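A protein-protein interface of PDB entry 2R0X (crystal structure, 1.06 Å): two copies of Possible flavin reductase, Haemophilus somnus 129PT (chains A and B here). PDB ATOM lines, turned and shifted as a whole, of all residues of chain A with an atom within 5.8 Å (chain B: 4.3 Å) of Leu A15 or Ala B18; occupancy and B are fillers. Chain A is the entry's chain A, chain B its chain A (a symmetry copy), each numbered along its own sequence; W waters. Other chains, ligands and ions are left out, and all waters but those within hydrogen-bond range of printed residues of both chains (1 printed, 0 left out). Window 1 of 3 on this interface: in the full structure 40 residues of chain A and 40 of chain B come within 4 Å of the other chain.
Water W1 lies within hydrogen-bond range of the backbone carbonyl oxygen of Ala A16 (2.8 Å) and the backbone NH of Ala B18 (3.0 Å).
Printed residues of chain B within 4 Å of Leu A15: Ala B18 (3.7 Å), His B20 (3.7 Å) and Ile B114 (3.7 Å).
Printed residues of chain A within 4 Å of Ala B18: Leu A15 and Ala A16.
Of the printed residues of chain A, Phe B116 touches Ala A11 (3.8 Å) and Met A12 (3.9 Å).
Of the printed residues of chain B, Ala A16 touches Ala B18.
The nearest printed residue of chain B that does not touch Leu A15 is Phe B116 (4.2 Å).
The nearest printed residue of chain A that does not touch Ala B18 is Ser A17 (5.5 Å).
The nearest printed residue of chain B that does not touch Ala A11 is His B20 (8.8 Å).
Of the 9 printed residues of chain B, 4 touch a printed residue of chain A.
Hydrophobic or aromatic side chains of chain B that line the printed part of chain A: Ala B18, His B20, Ile B114 and Phe B116.
Among the printed residues, no Asp or Glu carboxylate lies within 4 Å of a Lys or Arg side-chain nitrogen of the other chain.
The side-chain amide oxygen (OE1) of Gln A14 lies within hydrogen-bond range of the guanidinium group (NH2) of Arg A151, at 2.7 Å.
The backbone carbonyl oxygen of His B20 lies within hydrogen-bond range of the backbone NH of Ala B35 (2.8 Å).
Among the printed residues, merely in contact across the chains: Ala A11 with Ile B114 (3.5 Å), Ala A11 with Phe B116 (3.8 Å), Met A12 with Phe B116 (3.9 Å), Gln A14 with Ile B114 (3.6 Å), Leu A15 with Ala B18 (3.7 Å), Leu A15 with His B20 (3.7 Å), Leu A15 with Ile B114 (3.7 Å) and Ala A16 with Ala B18 (3.4 Å).
1 position is printed for both chains.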
ATOM      1  N   ALA A  11       6.438 -19.966   4.168  1.00  0.00           N
ATOM      2  CA  ALA A  11       5.365 -18.949   4.285  1.00  0.00           C
ATOM      3  C   ALA A  11       5.944 -17.552   4.158  1.00  0.00           C
ATOM      4  O   ALA A  11       5.423 -16.728   3.424  1.00  0.00           O
ATOM      5  CB  ALA A  11       4.543 -19.082   5.569  1.00  0.00           C
ATOM      6  N   MET A  12       7.072 -17.285   4.816  1.00  0.00           N
ATOM      7  CA  MET A  12       7.708 -15.961   4.713  1.00  0.00           C
ATOM      8  C   MET A  12       8.158 -15.646   3.298  1.00  0.00           C
ATOM      9  O   MET A  12       8.114 -14.480   2.874  1.00  0.00           O
ATOM     10  CB  MET A  12       8.897 -15.814   5.651  1.00  0.00           C
ATOM     11  CG  MET A  12       8.513 -15.695   7.133  1.00  0.00           C
ATOM     12  SD  MET A  12       7.295 -14.184   7.444  1.00  0.00           S
ATOM     13  CE  MET A  12       8.421 -12.743   6.814  1.00  0.00           C
ATOM     14  N   ALA A  13       8.563 -16.664   2.552  1.00  0.00           N
ATOM     15  CA  ALA A  13       8.944 -16.455   1.141  1.00  0.00           C
ATOM     16  C   ALA A  13       7.809 -15.839   0.321  1.00  0.00           C
ATOM     17  O   ALA A  13       8.048 -15.181  -0.693  1.00  0.00           O
ATOM     18  CB  ALA A  13       9.420 -17.747   0.508  1.00  0.00           C
ATOM     19  N   GLN A  14       6.561 -16.034   0.752  1.00  0.00           N
ATOM     20  CA  GLN A  14       5.419 -15.457   0.066  1.00  0.00           C
ATOM     21  C   GLN A  14       5.208 -13.973   0.416  1.00  0.00           C
ATOM     22  O   GLN A  14       4.536 -13.294  -0.338  1.00  0.00           O
ATOM     23  CB  GLN A  14       4.121 -16.230   0.399  1.00  0.00           C
ATOM     24  CG  GLN A  14       4.059 -17.745  -0.049  1.00  0.00           C
ATOM     25  CD  GLN A  14       3.979 -17.937  -1.563  1.00  0.00           C
ATOM     26  OE1 GLN A  14       3.383 -17.130  -2.278  1.00  0.00           O
ATOM     27  NE2 GLN A  14       4.583 -19.016  -2.051  1.00  0.00           N
ATOM     28  N   LEU A  15       5.767 -13.497   1.537  1.00  0.00           N
ATOM     29  CA  LEU A  15       5.498 -12.129   2.046  1.00  0.00           C
ATOM     30  C   LEU A  15       6.437 -11.126   1.385  1.00  0.00           C
ATOM     31  O   LEU A  15       7.634 -11.114   1.676  1.00  0.00           O
ATOM     32  CB  LEU A  15       5.655 -12.086   3.597  1.00  0.00           C
ATOM     33  CG  LEU A  15       4.924 -10.995   4.396  1.00  0.00           C
ATOM     34  CD1 LEU A  15       4.782 -11.382   5.872  1.00  0.00           C
ATOM     35  CD2 LEU A  15       5.625  -9.657   4.287  1.00  0.00           C
ATOM     36  N   ALA A  16       5.891 -10.317   0.469  1.00  0.00           N
ATOM     37  CA  ALA A  16       6.642  -9.351  -0.298  1.00  0.00           C
ATOM     38  C   ALA A  16       7.276  -8.343   0.647  1.00  0.00           C
ATOM     39  O   ALA A  16       6.610  -7.838   1.556  1.00  0.00           O
ATOM     40  CB  ALA A  16       5.712  -8.599  -1.236  1.00  0.00           C
ATOM     41  N   SER A  17       8.508  -7.978   0.374  1.00  0.00           N
ATOM     42  CA  SER A  17       9.149  -7.000   1.223  1.00  0.00           C
ATOM     43  C   SER A  17      10.045  -6.105   0.414  1.00  0.00           C
ATOM     44  O   SER A  17      10.651  -6.510  -0.572  1.00  0.00           O
ATOM     45  CB  SER A  17       9.963  -7.712   2.287  1.00  0.00           C
ATOM     46  OG  SER A  17      10.632  -6.852   3.171  1.00  0.00           O
ATOM     47  N   TYR A 150      11.457  -8.140  -2.697  1.00  0.00           N
ATOM     48  CA  TYR A 150      11.871  -9.553  -2.622  1.00  0.00           C
ATOM     49  C   TYR A 150      10.615 -10.397  -2.290  1.00  0.00           C
ATOM     50  O   TYR A 150       9.889 -10.082  -1.351  1.00  0.00           O
ATOM     51  CB  TYR A 150      12.920  -9.699  -1.539  1.00  0.00           C
ATOM     52  CG  TYR A 150      13.604 -11.030  -1.408  1.00  0.00           C
ATOM     53  CD1 TYR A 150      14.311 -11.583  -2.455  1.00  0.00           C
ATOM     54  CD2 TYR A 150      13.534 -11.740  -0.202  1.00  0.00           C
ATOM     55  CE1 TYR A 150      14.950 -12.816  -2.307  1.00  0.00           C
ATOM     56  CE2 TYR A 150      14.176 -12.940  -0.046  1.00  0.00           C
ATOM     57  CZ  TYR A 150      14.892 -13.481  -1.076  1.00  0.00           C
ATOM     58  OH  TYR A 150      15.524 -14.707  -0.859  1.00  0.00           O
ATOM     59  N   ARG A 151      10.349 -11.398  -3.114  1.00  0.00           N
ATOM     60  CA  ARG A 151       9.211 -12.284  -2.905  1.00  0.00           C
ATOM     61  C   ARG A 151       9.492 -13.577  -3.682  1.00  0.00           C
ATOM     62  O   ARG A 151      10.020 -13.558  -4.779  1.00  0.00           O
ATOM     63  CB  ARG A 151       7.884 -11.666  -3.380  1.00  0.00           C
ATOM     64  CG  ARG A 151       6.708 -12.486  -2.878  1.00  0.00           C
ATOM     65  CD  ARG A 151       5.432 -12.171  -3.562  1.00  0.00           C
ATOM     66  NE  ARG A 151       4.486 -13.230  -3.212  1.00  0.00           N
ATOM     67  CZ  ARG A 151       3.655 -13.839  -4.051  1.00  0.00           C
ATOM     68  NH1 ARG A 151       3.533 -13.414  -5.299  1.00  0.00           N
ATOM     69  NH2 ARG A 151       2.925 -14.863  -3.619  1.00  0.00           N
ATOM     70  N   SER B  17       5.354  -2.131   0.641  1.00  0.00           N
ATOM     71  CA  SER B  17       5.014  -3.035   1.715  1.00  0.00           C
ATOM     72  C   SER B  17       3.924  -3.978   1.288  1.00  0.00           C
ATOM     73  O   SER B  17       3.042  -3.642   0.505  1.00  0.00           O
ATOM     74  CB  SER B  17       4.553  -2.235   2.920  1.00  0.00           C
ATOM     75  OG  SER B  17       4.196  -3.018   4.028  1.00  0.00           O
ATOM     76  N   ALA B  18       4.015  -5.171   1.850  1.00  0.00           N
ATOM     77  CA  ALA B  18       2.920  -6.119   1.859  1.00  0.00           C
ATOM     78  C   ALA B  18       1.792  -5.529   2.687  1.00  0.00           C
ATOM     79  O   ALA B  18       1.967  -4.644   3.493  1.00  0.00           O
ATOM     80  CB  ALA B  18       3.339  -7.469   2.386  1.00  0.00           C
ATOM     81  N   VAL B  19       0.575  -6.005   2.445  1.00  0.00           N
ATOM     82  CA  VAL B  19      -0.618  -5.546   3.104  1.00  0.00           C
ATOM     83  C   VAL B  19      -1.278  -6.721   3.783  1.00  0.00           C
ATOM     84  O   VAL B  19      -1.414  -7.793   3.219  1.00  0.00           O
ATOM     85  CB  VAL B  19      -1.596  -4.907   2.104  1.00  0.00           C
ATOM     86  CG1 VAL B  19      -2.805  -4.319   2.840  1.00  0.00           C
ATOM     87  CG2 VAL B  19      -0.927  -3.814   1.264  1.00  0.00           C
ATOM     88  N   HIS B  20      -1.678  -6.530   5.024  1.00  0.00           N
ATOM     89  CA  HIS B  20      -2.249  -7.583   5.852  1.00  0.00           C
ATOM     90  C   HIS B  20      -3.524  -7.074   6.508  1.00  0.00           C
ATOM     91  O   HIS B  20      -3.692  -5.857   6.760  1.00  0.00           O
ATOM     92  CB  HIS B  20      -1.274  -7.970   6.969  1.00  0.00           C
ATOM     93  CG  HIS B  20       0.124  -8.096   6.551  1.00  0.00           C
ATOM     94  ND1 HIS B  20       0.660  -9.278   6.106  1.00  0.00           N
ATOM     95  CD2 HIS B  20       1.080  -7.149   6.478  1.00  0.00           C
ATOM     96  CE1 HIS B  20       1.906  -9.030   5.745  1.00  0.00           C
ATOM     97  NE2 HIS B  20       2.187  -7.749   5.960  1.00  0.00           N
ATOM     98  N   ALA B  35      -3.017  -3.543   8.196  1.00  0.00           N
ATOM     99  CA  ALA B  35      -1.662  -3.171   8.637  1.00  0.00           C
ATOM    100  C   ALA B  35      -0.651  -3.401   7.546  1.00  0.00           C
ATOM    101  O   ALA B  35      -0.720  -4.367   6.799  1.00  0.00           O
ATOM    102  CB  ALA B  35      -1.264  -4.016   9.843  1.00  0.00           C
ATOM    103  N   SER B  36       0.338  -2.522   7.517  1.00  0.00           N
ATOM    104  CA  SER B  36       1.544  -2.745   6.734  1.00  0.00           C
ATOM    105  C   SER B  36       2.784  -3.000   7.610  1.00  0.00           C
ATOM    106  O   SER B  36       3.781  -3.583   7.137  1.00  0.00           O
ATOM    107  CB  SER B  36       1.823  -1.552   5.827  1.00  0.00           C
ATOM    108  OG  SER B  36       1.750  -0.335   6.558  1.00  0.00           O
ATOM    109  N   ILE B 114      -1.459 -15.611   2.689  1.00  0.00           N
ATOM    110  CA  ILE B 114      -0.835 -16.326   3.805  1.00  0.00           C
ATOM    111  C   ILE B 114      -1.652 -16.030   5.043  1.00  0.00           C
ATOM    112  O   ILE B 114      -2.193 -14.943   5.157  1.00  0.00           O
ATOM    113  CB  ILE B 114       0.650 -15.850   4.104  1.00  0.00           C
ATOM    114  CG1 ILE B 114       1.369 -15.274   2.876  1.00  0.00           C
ATOM    115  CG2 ILE B 114       1.430 -16.995   4.702  1.00  0.00           C
ATOM    116  CD1 ILE B 114       2.656 -14.544   3.205  1.00  0.00           C
ATOM    117  N   PHE B 116      -1.073 -16.384   9.262  1.00  0.00           N
ATOM    118  CA  PHE B 116      -0.232 -16.712  10.411  1.00  0.00           C
ATOM    119  C   PHE B 116      -1.035 -16.520  11.684  1.00  0.00           C
ATOM    120  O   PHE B 116      -1.420 -15.419  12.018  1.00  0.00           O
ATOM    121  CB  PHE B 116       0.976 -15.778  10.504  1.00  0.00           C
ATOM    122  CG  PHE B 116       1.849 -15.680   9.289  1.00  0.00           C
ATOM    123  CD1 PHE B 116       1.590 -14.755   8.299  1.00  0.00           C
ATOM    124  CD2 PHE B 116       2.967 -16.456   9.168  1.00  0.00           C
ATOM    125  CE1 PHE B 116       2.452 -14.613   7.204  1.00  0.00           C
ATOM    126  CE2 PHE B 116       3.844 -16.282   8.080  1.00  0.00           C
ATOM    127  CZ  PHE B 116       3.549 -15.362   7.117  1.00  0.00           C
ATOM    128  N   LEU B 148      -0.538  -8.522  -2.812  1.00  0.00           N
ATOM    129  CA  LEU B 148      -0.859  -7.102  -2.798  1.00  0.00           C
ATOM    130  C   LEU B 148       0.296  -6.336  -2.151  1.00  0.00           C
ATOM    131  O   LEU B 148       0.720  -6.634  -1.048  1.00  0.00           O
ATOM    132  CB  LEU B 148      -2.114  -6.852  -1.966  1.00  0.00           C
ATOM    133  CG  LEU B 148      -2.708  -5.466  -2.057  1.00  0.00           C
ATOM    134  CD1 LEU B 148      -3.135  -5.088  -3.489  1.00  0.00           C
ATOM    135  CD2 LEU B 148      -3.883  -5.317  -1.097  1.00  0.00           C
HETATM  136  O   HOH W   1       6.353  -5.886   3.538  1.00  0.00           O
